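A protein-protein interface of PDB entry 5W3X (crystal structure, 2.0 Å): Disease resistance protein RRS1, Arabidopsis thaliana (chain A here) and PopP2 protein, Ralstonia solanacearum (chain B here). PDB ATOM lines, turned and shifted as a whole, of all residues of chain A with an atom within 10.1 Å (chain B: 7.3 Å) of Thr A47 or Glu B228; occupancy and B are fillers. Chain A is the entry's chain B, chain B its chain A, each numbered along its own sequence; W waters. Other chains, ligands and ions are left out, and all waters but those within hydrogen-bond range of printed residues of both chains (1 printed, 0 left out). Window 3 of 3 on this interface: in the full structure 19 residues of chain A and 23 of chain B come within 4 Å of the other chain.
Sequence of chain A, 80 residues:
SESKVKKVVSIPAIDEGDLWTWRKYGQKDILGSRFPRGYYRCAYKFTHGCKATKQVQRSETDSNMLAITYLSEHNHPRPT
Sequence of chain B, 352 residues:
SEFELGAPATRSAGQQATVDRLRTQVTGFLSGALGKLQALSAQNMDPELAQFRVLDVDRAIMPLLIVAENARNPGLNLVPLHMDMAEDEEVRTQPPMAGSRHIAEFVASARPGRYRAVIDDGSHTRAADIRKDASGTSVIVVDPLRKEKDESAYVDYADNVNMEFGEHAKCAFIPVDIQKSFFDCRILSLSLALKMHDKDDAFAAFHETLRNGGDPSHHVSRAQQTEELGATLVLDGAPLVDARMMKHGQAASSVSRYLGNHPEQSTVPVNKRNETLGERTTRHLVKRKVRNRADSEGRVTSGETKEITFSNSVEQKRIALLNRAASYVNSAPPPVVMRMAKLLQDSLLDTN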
ATOM      1  N   THR A  21      -1.250   7.250 -10.737  1.00  0.00           N
ATOM      2  CA  THR A  21      -1.526   6.794 -12.095  1.00  0.00           C
ATOM      3  C   THR A  21      -0.591   7.464 -13.101  1.00  0.00           C
ATOM      4  O   THR A  21      -0.319   8.663 -13.009  1.00  0.00           O
ATOM      5  CB  THR A  21      -2.984   7.066 -12.500  1.00  0.00           C
ATOM      6  OG1 THR A  21      -3.313   8.432 -12.223  1.00  0.00           O
ATOM      7  CG2 THR A  21      -3.923   6.153 -11.730  1.00  0.00           C
ATOM      8  N   TRP A  22      -0.104   6.675 -14.058  1.00  0.00           N
ATOM      9  CA  TRP A  22       0.968   7.101 -14.953  1.00  0.00           C
ATOM     10  C   TRP A  22       0.697   6.771 -16.423  1.00  0.00           C
ATOM     11  O   TRP A  22       0.007   5.803 -16.728  1.00  0.00           O
ATOM     12  CB  TRP A  22       2.276   6.442 -14.523  1.00  0.00           C
ATOM     13  CG  TRP A  22       2.633   6.677 -13.074  1.00  0.00           C
ATOM     14  CD1 TRP A  22       2.396   5.830 -12.030  1.00  0.00           C
ATOM     15  CD2 TRP A  22       3.305   7.816 -12.518  1.00  0.00           C
ATOM     16  NE1 TRP A  22       2.865   6.374 -10.861  1.00  0.00           N
ATOM     17  CE2 TRP A  22       3.430   7.591 -11.132  1.00  0.00           C
ATOM     18  CE3 TRP A  22       3.806   9.005 -13.055  1.00  0.00           C
ATOM     19  CZ2 TRP A  22       4.034   8.509 -10.279  1.00  0.00           C
ATOM     20  CZ3 TRP A  22       4.407   9.915 -12.204  1.00  0.00           C
ATOM     21  CH2 TRP A  22       4.515   9.662 -10.834  1.00  0.00           C
ATOM     22  N   ARG A  23       1.232   7.598 -17.322  1.00  0.00           N
ATOM     23  CA  ARG A  23       1.218   7.325 -18.764  1.00  0.00           C
ATOM     24  C   ARG A  23       2.666   7.349 -19.270  1.00  0.00           C
ATOM     25  O   ARG A  23       3.533   7.952 -18.649  1.00  0.00           O
ATOM     26  CB  ARG A  23       0.361   8.338 -19.529  1.00  0.00           C
ATOM     27  CG  ARG A  23      -1.099   8.402 -19.063  1.00  0.00           C
ATOM     28  CD  ARG A  23      -1.876   7.111 -19.339  1.00  0.00           C
ATOM     29  NE  ARG A  23      -3.011   7.001 -18.423  1.00  0.00           N
ATOM     30  CZ  ARG A  23      -4.204   7.542 -18.646  1.00  0.00           C
ATOM     31  NH1 ARG A  23      -4.423   8.222 -19.762  1.00  0.00           N
ATOM     32  NH2 ARG A  23      -5.181   7.405 -17.759  1.00  0.00           N
ATOM     33  N   LYS A  24       2.920   6.682 -20.388  1.00  0.00           N
ATOM     34  CA  LYS A  24       4.273   6.539 -20.910  1.00  0.00           C
ATOM     35  C   LYS A  24       4.822   7.835 -21.521  1.00  0.00           C
ATOM     36  O   LYS A  24       4.090   8.606 -22.153  1.00  0.00           O
ATOM     37  CB  LYS A  24       4.298   5.429 -21.950  1.00  0.00           C
ATOM     38  CG  LYS A  24       5.613   4.689 -22.032  1.00  0.00           C
ATOM     39  CD  LYS A  24       5.951   4.020 -20.717  1.00  0.00           C
ATOM     40  CE  LYS A  24       7.296   3.318 -20.781  1.00  0.00           C
ATOM     41  NZ  LYS A  24       7.297   2.154 -21.717  1.00  0.00           N
ATOM     42  N   ARG A  41       5.064   9.954 -16.945  1.00  0.00           N
ATOM     43  CA  ARG A  41       4.583  11.245 -16.446  1.00  0.00           C
ATOM     44  C   ARG A  41       3.191  10.988 -15.900  1.00  0.00           C
ATOM     45  O   ARG A  41       2.646   9.916 -16.155  1.00  0.00           O
ATOM     46  CB  ARG A  41       4.604  12.297 -17.560  1.00  0.00           C
ATOM     47  CG  ARG A  41       3.892  11.891 -18.866  1.00  0.00           C
ATOM     48  CD  ARG A  41       2.419  12.333 -18.889  1.00  0.00           C
ATOM     49  NE  ARG A  41       1.799  12.112 -20.192  1.00  0.00           N
ATOM     50  CZ  ARG A  41       0.494  11.957 -20.388  1.00  0.00           C
ATOM     51  NH1 ARG A  41      -0.340  11.970 -19.361  1.00  0.00           N
ATOM     52  NH2 ARG A  41       0.026  11.767 -21.613  1.00  0.00           N
ATOM     53  N   CYS A  42       2.640  11.890 -15.090  1.00  0.00           N
ATOM     54  CA  CYS A  42       1.341  11.638 -14.451  1.00  0.00           C
ATOM     55  C   CYS A  42       0.143  11.585 -15.409  1.00  0.00           C
ATOM     56  O   CYS A  42       0.088  12.306 -16.400  1.00  0.00           O
ATOM     57  CB  CYS A  42       1.047  12.694 -13.377  1.00  0.00           C
ATOM     58  SG  CYS A  42      -0.504  12.351 -12.479  1.00  0.00           S
ATOM     59  N   ALA A  43      -0.829  10.738 -15.095  1.00  0.00           N
ATOM     60  CA  ALA A  43      -2.044  10.657 -15.904  1.00  0.00           C
ATOM     61  C   ALA A  43      -2.845  11.961 -15.869  1.00  0.00           C
ATOM     62  O   ALA A  43      -3.708  12.185 -16.719  1.00  0.00           O
ATOM     63  CB  ALA A  43      -2.911   9.500 -15.439  1.00  0.00           C
ATOM     64  N   TYR A  44      -2.558  12.823 -14.896  1.00  0.00           N
ATOM     65  CA  TYR A  44      -3.255  14.103 -14.777  1.00  0.00           C
ATOM     66  C   TYR A  44      -2.353  15.277 -15.148  1.00  0.00           C
ATOM     67  O   TYR A  44      -2.560  16.402 -14.687  1.00  0.00           O
ATOM     68  CB  TYR A  44      -3.788  14.289 -13.352  1.00  0.00           C
ATOM     69  CG  TYR A  44      -4.668  13.151 -12.898  1.00  0.00           C
ATOM     70  CD1 TYR A  44      -6.003  13.076 -13.290  1.00  0.00           C
ATOM     71  CD2 TYR A  44      -4.161  12.139 -12.092  1.00  0.00           C
ATOM     72  CE1 TYR A  44      -6.815  12.025 -12.880  1.00  0.00           C
ATOM     73  CE2 TYR A  44      -4.960  11.085 -11.678  1.00  0.00           C
ATOM     74  CZ  TYR A  44      -6.283  11.031 -12.072  1.00  0.00           C
ATOM     75  OH  TYR A  44      -7.066   9.976 -11.653  1.00  0.00           O
ATOM     76  N   LYS A  45      -1.378  15.024 -16.016  1.00  0.00           N
ATOM     77  CA  LYS A  45      -0.517  16.091 -16.502  1.00  0.00           C
ATOM     78  C   LYS A  45      -1.310  17.146 -17.261  1.00  0.00           C
ATOM     79  O   LYS A  45      -1.058  18.337 -17.131  1.00  0.00           O
ATOM     80  CB  LYS A  45       0.576  15.531 -17.411  1.00  0.00           C
ATOM     81  CG  LYS A  45       1.456  16.606 -18.050  1.00  0.00           C
ATOM     82  CD  LYS A  45       2.603  15.988 -18.836  1.00  0.00           C
ATOM     83  CE  LYS A  45       3.500  17.049 -19.438  1.00  0.00           C
ATOM     84  NZ  LYS A  45       3.960  18.006 -18.399  1.00  0.00           N
ATOM     85  N   PHE A  46      -2.253  16.696 -18.073  1.00  0.00           N
ATOM     86  CA  PHE A  46      -2.981  17.588 -18.960  1.00  0.00           C
ATOM     87  C   PHE A  46      -4.154  18.237 -18.228  1.00  0.00           C
ATOM     88  O   PHE A  46      -4.303  19.461 -18.229  1.00  0.00           O
ATOM     89  CB  PHE A  46      -3.447  16.811 -20.193  1.00  0.00           C
ATOM     90  CG  PHE A  46      -4.241  17.623 -21.180  1.00  0.00           C
ATOM     91  CD1 PHE A  46      -3.644  18.651 -21.896  1.00  0.00           C
ATOM     92  CD2 PHE A  46      -5.576  17.324 -21.428  1.00  0.00           C
ATOM     93  CE1 PHE A  46      -4.373  19.387 -22.817  1.00  0.00           C
ATOM     94  CE2 PHE A  46      -6.309  18.056 -22.352  1.00  0.00           C
ATOM     95  CZ  PHE A  46      -5.707  19.088 -23.047  1.00  0.00           C
ATOM     96  N   THR A  47      -4.970  17.408 -17.585  1.00  0.00           N
ATOM     97  CA  THR A  47      -6.166  17.888 -16.902  1.00  0.00           C
ATOM     98  C   THR A  47      -5.830  18.788 -15.715  1.00  0.00           C
ATOM     99  O   THR A  47      -6.512  19.780 -15.474  1.00  0.00           O
ATOM    100  CB  THR A  47      -7.045  16.711 -16.415  1.00  0.00           C
ATOM    101  OG1 THR A  47      -6.268  15.826 -15.597  1.00  0.00           O
ATOM    102  CG2 THR A  47      -7.592  15.938 -17.596  1.00  0.00           C
ATOM    103  N   HIS A  48      -4.776  18.455 -14.981  1.00  0.00           N
ATOM    104  CA  HIS A  48      -4.454  19.198 -13.767  1.00  0.00           C
ATOM    105  C   HIS A  48      -3.120  19.935 -13.792  1.00  0.00           C
ATOM    106  O   HIS A  48      -2.757  20.592 -12.812  1.00  0.00           O
ATOM    107  CB  HIS A  48      -4.469  18.250 -12.572  1.00  0.00           C
ATOM    108  CG  HIS A  48      -5.838  17.799 -12.183  1.00  0.00           C
ATOM    109  ND1 HIS A  48      -6.524  16.823 -12.872  1.00  0.00           N
ATOM    110  CD2 HIS A  48      -6.662  18.207 -11.188  1.00  0.00           C
ATOM    111  CE1 HIS A  48      -7.706  16.637 -12.309  1.00  0.00           C
ATOM    112  NE2 HIS A  48      -7.815  17.466 -11.287  1.00  0.00           N
ATOM    113  N   GLY A  49      -2.388  19.827 -14.896  1.00  0.00           N
ATOM    114  CA  GLY A  49      -1.069  20.432 -14.982  1.00  0.00           C
ATOM    115  C   GLY A  49      -0.030  19.763 -14.091  1.00  0.00           C
ATOM    116  O   GLY A  49       1.042  20.326 -13.870  1.00  0.00           O
ATOM    117  N   CYS A  50      -0.327  18.560 -13.596  1.00  0.00           N
ATOM    118  CA  CYS A  50       0.576  17.863 -12.674  1.00  0.00           C
ATOM    119  C   CYS A  50       1.940  17.621 -13.322  1.00  0.00           C
ATOM    120  O   CYS A  50       2.021  17.182 -14.475  1.00  0.00           O
ATOM    121  CB  CYS A  50      -0.042  16.535 -12.210  1.00  0.00           C
ATOM    122  SG  CYS A  50       0.969  15.589 -11.004  1.00  0.00           S
ATOM    123  N   LYS A  51       3.003  17.912 -12.578  1.00  0.00           N
ATOM    124  CA  LYS A  51       4.360  17.874 -13.127  1.00  0.00           C
ATOM    125  C   LYS A  51       5.138  16.613 -12.742  1.00  0.00           C
ATOM    126  O   LYS A  51       6.303  16.437 -13.123  1.00  0.00           O
ATOM    127  CB  LYS A  51       5.133  19.117 -12.680  1.00  0.00           C
ATOM    128  CG  LYS A  51       4.631  20.409 -13.295  1.00  0.00           C
ATOM    129  CD  LYS A  51       5.492  21.589 -12.868  1.00  0.00           C
ATOM    130  CE  LYS A  51       5.093  22.858 -13.604  1.00  0.00           C
ATOM    131  NZ  LYS A  51       5.957  24.014 -13.233  1.00  0.00           N
ATOM    132  N   ASN A  75       0.151  17.574  -7.831  1.00  0.00           N
ATOM    133  CA  ASN A  75      -0.671  18.704  -7.388  1.00  0.00           C
ATOM    134  C   ASN A  75      -2.131  18.305  -7.232  1.00  0.00           C
ATOM    135  O   ASN A  75      -3.035  19.073  -7.552  1.00  0.00           O
ATOM    136  CB  ASN A  75      -0.546  19.886  -8.361  1.00  0.00           C
ATOM    137  CG  ASN A  75      -1.112  19.583  -9.747  1.00  0.00           C
ATOM    138  OD1 ASN A  75      -1.506  18.453 -10.046  1.00  0.00           O
ATOM    139  ND2 ASN A  75      -1.140  20.600 -10.606  1.00  0.00           N
ATOM    140  N   HIS A  76      -2.356  17.101  -6.724  1.00  0.00           N
ATOM    141  CA  HIS A  76      -3.706  16.568  -6.565  1.00  0.00           C
ATOM    142  C   HIS A  76      -3.658  15.358  -5.637  1.00  0.00           C
ATOM    143  O   HIS A  76      -2.605  14.739  -5.486  1.00  0.00           O
ATOM    144  CB  HIS A  76      -4.291  16.186  -7.924  1.00  0.00           C
ATOM    145  CG  HIS A  76      -3.469  15.180  -8.659  1.00  0.00           C
ATOM    146  ND1 HIS A  76      -3.667  13.821  -8.530  1.00  0.00           N
ATOM    147  CD2 HIS A  76      -2.425  15.330  -9.509  1.00  0.00           C
ATOM    148  CE1 HIS A  76      -2.788  13.180  -9.279  1.00  0.00           C
ATOM    149  NE2 HIS A  76      -2.027  14.072  -9.886  1.00  0.00           N
ATOM    150  N   VAL B 155      -0.245   6.103 -27.679  1.00  0.00           N
ATOM    151  CA  VAL B 155      -1.287   7.112 -27.456  1.00  0.00           C
ATOM    152  C   VAL B 155      -0.679   8.179 -26.565  1.00  0.00           C
ATOM    153  O   VAL B 155      -0.713   9.375 -26.887  1.00  0.00           O
ATOM    154  CB  VAL B 155      -2.566   6.501 -26.817  1.00  0.00           C
ATOM    155  CG1 VAL B 155      -3.537   7.580 -26.324  1.00  0.00           C
ATOM    156  CG2 VAL B 155      -3.259   5.597 -27.813  1.00  0.00           C
ATOM    157  N   ASP B 156      -0.037   7.724 -25.489  1.00  0.00           N
ATOM    158  CA  ASP B 156       0.590   8.634 -24.545  1.00  0.00           C
ATOM    159  C   ASP B 156       1.611   9.518 -25.273  1.00  0.00           C
ATOM    160  O   ASP B 156       1.574  10.745 -25.156  1.00  0.00           O
ATOM    161  CB  ASP B 156       1.264   7.862 -23.405  1.00  0.00           C
ATOM    162  CG  ASP B 156       0.319   6.890 -22.704  1.00  0.00           C
ATOM    163  OD1 ASP B 156      -0.918   7.056 -22.827  1.00  0.00           O
ATOM    164  OD2 ASP B 156       0.828   5.979 -22.002  1.00  0.00           O
ATOM    165  N   ASP B 159       0.082  12.164 -27.376  1.00  0.00           N
ATOM    166  CA  ASP B 159      -0.487  13.218 -26.545  1.00  0.00           C
ATOM    167  C   ASP B 159       0.643  14.119 -26.048  1.00  0.00           C
ATOM    168  O   ASP B 159       0.531  15.358 -26.077  1.00  0.00           O
ATOM    169  CB  ASP B 159      -1.275  12.627 -25.375  1.00  0.00           C
ATOM    170  CG  ASP B 159      -2.682  12.158 -25.783  1.00  0.00           C
ATOM    171  OD1 ASP B 159      -3.152  12.514 -26.887  1.00  0.00           O
ATOM    172  OD2 ASP B 159      -3.320  11.438 -24.984  1.00  0.00           O
ATOM    173  N   MET B 163       0.912  18.059 -26.595  1.00  0.00           N
ATOM    174  CA  MET B 163       0.642  19.094 -25.607  1.00  0.00           C
ATOM    175  C   MET B 163       1.842  20.034 -25.524  1.00  0.00           C
ATOM    176  O   MET B 163       1.721  21.140 -25.019  1.00  0.00           O
ATOM    177  CB  MET B 163       0.235  18.522 -24.241  1.00  0.00           C
ATOM    178  CG  MET B 163       1.168  17.615 -23.489  1.00  0.00           C
ATOM    179  SD  MET B 163       0.247  16.918 -22.071  1.00  0.00           S
ATOM    180  CE  MET B 163      -0.158  15.273 -22.649  1.00  0.00           C
ATOM    181  N   GLU B 167      -2.377  22.523 -27.373  1.00  0.00           N
ATOM    182  CA  GLU B 167      -3.669  21.889 -27.652  1.00  0.00           C
ATOM    183  C   GLU B 167      -4.235  22.135 -29.039  1.00  0.00           C
ATOM    184  O   GLU B 167      -4.891  21.266 -29.605  1.00  0.00           O
ATOM    185  CB  GLU B 167      -4.730  22.379 -26.664  1.00  0.00           C
ATOM    186  CG  GLU B 167      -4.577  21.946 -25.242  1.00  0.00           C
ATOM    187  CD  GLU B 167      -5.691  22.524 -24.392  1.00  0.00           C
ATOM    188  OE1 GLU B 167      -6.755  22.832 -24.969  1.00  0.00           O
ATOM    189  OE2 GLU B 167      -5.503  22.685 -23.167  1.00  0.00           O
ATOM    190  N   GLN B 225      -7.418   8.730 -33.775  1.00  0.00           N
ATOM    191  CA  GLN B 225      -7.250   9.911 -32.921  1.00  0.00           C
ATOM    192  C   GLN B 225      -7.215   9.495 -31.466  1.00  0.00           C
ATOM    193  O   GLN B 225      -7.945   8.590 -31.060  1.00  0.00           O
ATOM    194  CB  GLN B 225      -8.384  10.910 -33.116  1.00  0.00           C
ATOM    195  CG  GLN B 225      -8.963  10.918 -34.487  1.00  0.00           C
ATOM    196  CD  GLN B 225      -8.654  12.198 -35.181  1.00  0.00           C
ATOM    197  OE1 GLN B 225      -7.508  12.436 -35.561  1.00  0.00           O
ATOM    198  NE2 GLN B 225      -9.664  13.055 -35.334  1.00  0.00           N
ATOM    199  N   THR B 226      -6.374  10.155 -30.682  1.00  0.00           N
ATOM    200  CA  THR B 226      -6.304   9.874 -29.259  1.00  0.00           C
ATOM    201  C   THR B 226      -7.475  10.534 -28.545  1.00  0.00           C
ATOM    202  O   THR B 226      -8.001  11.540 -29.015  1.00  0.00           O
ATOM    203  CB  THR B 226      -5.019  10.377 -28.649  1.00  0.00           C
ATOM    204  OG1 THR B 226      -5.033  11.805 -28.637  1.00  0.00           O
ATOM    205  CG2 THR B 226      -3.800   9.878 -29.463  1.00  0.00           C
ATOM    206  N   GLU B 227      -7.841   9.997 -27.390  1.00  0.00           N
ATOM    207  CA  GLU B 227      -9.037  10.445 -26.690  1.00  0.00           C
ATOM    208  C   GLU B 227      -8.804  11.792 -26.010  1.00  0.00           C
ATOM    209  O   GLU B 227      -9.687  12.651 -26.000  1.00  0.00           O
ATOM    210  CB  GLU B 227      -9.472   9.395 -25.664  1.00  0.00           C
ATOM    211  CG  GLU B 227     -10.975   9.275 -25.479  1.00  0.00           C
ATOM    212  CD  GLU B 227     -11.698   8.894 -26.763  1.00  0.00           C
ATOM    213  OE1 GLU B 227     -11.533   7.743 -27.225  1.00  0.00           O
ATOM    214  OE2 GLU B 227     -12.427   9.754 -27.311  1.00  0.00           O
ATOM    215  N   GLU B 228      -7.613  11.997 -25.455  1.00  0.00           N
ATOM    216  CA  GLU B 228      -7.402  13.174 -24.624  1.00  0.00           C
ATOM    217  C   GLU B 228      -7.050  14.429 -25.430  1.00  0.00           C
ATOM    218  O   GLU B 228      -7.553  15.509 -25.145  1.00  0.00           O
ATOM    219  CB  GLU B 228      -6.316  12.896 -23.581  1.00  0.00           C
ATOM    220  CG  GLU B 228      -6.244  13.959 -22.487  1.00  0.00           C
ATOM    221  CD  GLU B 228      -5.425  13.519 -21.282  1.00  0.00           C
ATOM    222  OE1 GLU B 228      -4.767  12.460 -21.362  1.00  0.00           O
ATOM    223  OE2 GLU B 228      -5.444  14.232 -20.255  1.00  0.00           O
ATOM    224  N   LEU B 229      -6.197  14.297 -26.441  1.00  0.00           N
ATOM    225  CA  LEU B 229      -5.784  15.473 -27.210  1.00  0.00           C
ATOM    226  C   LEU B 229      -6.276  15.441 -28.653  1.00  0.00           C
ATOM    227  O   LEU B 229      -6.165  16.435 -29.362  1.00  0.00           O
ATOM    228  CB  LEU B 229      -4.262  15.618 -27.181  1.00  0.00           C
ATOM    229  CG  LEU B 229      -3.848  16.492 -25.999  1.00  0.00           C
ATOM    230  CD1 LEU B 229      -3.168  15.682 -24.914  1.00  0.00           C
ATOM    231  CD2 LEU B 229      -2.984  17.647 -26.470  1.00  0.00           C
ATOM    232  N   GLY B 230      -6.823  14.307 -29.091  1.00  0.00           N
ATOM    233  CA  GLY B 230      -7.257  14.196 -30.470  1.00  0.00           C
ATOM    234  C   GLY B 230      -6.105  14.171 -31.467  1.00  0.00           C
ATOM    235  O   GLY B 230      -6.306  14.401 -32.664  1.00  0.00           O
ATOM    236  N   ALA B 231      -4.894  13.924 -30.970  1.00  0.00           N
ATOM    237  CA  ALA B 231      -3.729  13.702 -31.836  1.00  0.00           C
ATOM    238  C   ALA B 231      -3.963  12.490 -32.730  1.00  0.00           C
ATOM    239  O   ALA B 231      -4.633  11.548 -32.322  1.00  0.00           O
ATOM    240  CB  ALA B 231      -2.499  13.487 -31.005  1.00  0.00           C
HETATM  241  O   HOH W   1      -2.581  11.314 -22.652  1.00  0.00           O
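Water W1 lies within hydrogen-bond range of OD2 of Asp B159 (2.4 Å), OE1 of Glu B228 (2.8 Å) and NH2 of Arg A41 (2.8 Å).
The backbone NH (N) of Arg A23 sits at hydrogen-bond distance from the backbone carbonyl oxygen (O) of Arg A41, at 3.0 Å. OG1 of Thr A47 sits at hydrogen-bond distance from ND1 of His A48 (2.9 Å).
CB of Arg A23 touches OD2 of Asp B156, 3.4 Å away. NH2 of Arg A41 touches O of Asp B156, at 3.999 Å. Met B163 touches Arg A41 (CE to NH2, 3.7 Å). Phe A46 touches Glu B167. Glu B228 touches Phe A46. OE2 of Glu B228 touches CG2 of Thr A47, 3.8 Å away.
Of the 17 printed residues of chain A, 5 touch a printed residue of chain B. Hydrophobic or aromatic side chains of chain A that line the printed part of chain B: Phe A46. Printed residues of chain B that touch a printed residue of chain A: Asp B156, Met B163, Glu B167 and Glu B228. Hydrophobic or aromatic side chains of chain B that line the printed part of chain A: Met B163. Among the printed residues, no Asp or Glu carboxylate lies within 4 Å of a Lys or Arg side-chain nitrogen of the other chain.
Printed residues of chain B within 4 Å of Thr A47: Glu B228 (3.8 Å). Glu B228 touches just these residues of chain A: Phe A46 (3.3 Å) and Thr A47 (3.8 Å). Thr B226 touches none of the printed residues of chain A. No residue of chain A comes within 4 Å of Glu B227. Leu B229 touches none of the printed residues of chain A. Of the printed residues of chain A, Asp B156 touches Arg A23, Lys A24 and Arg A41. Of the printed residues of chain B, Phe A46 touches Glu B167 and Glu B228. Printed residues of chain A within 4 Å of Met B163: Arg A41 (3.7 Å). Printed residues of chain B within 4 Å of Arg A41: Asp B156 and Met B163. Of the printed residues of chain A, Glu B167 touches Phe A46 (3.5 Å). His A48 touches none of the printed residues of chain B. The nearest residue of chain B that does not touch Thr A47 is Met B163 (6.9 Å). The nearest residue of chain A that does not touch Glu B228 is Ala A43 (4.4 Å). The nearest printed residue of chain B that does not touch Phe A46 is Met B163 (4.1 Å).
The side-chain carboxylate (OD2) of Asp B156 sits at hydrogen-bond distance from the backbone NH (N) of Lys A24 (2.7 Å).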
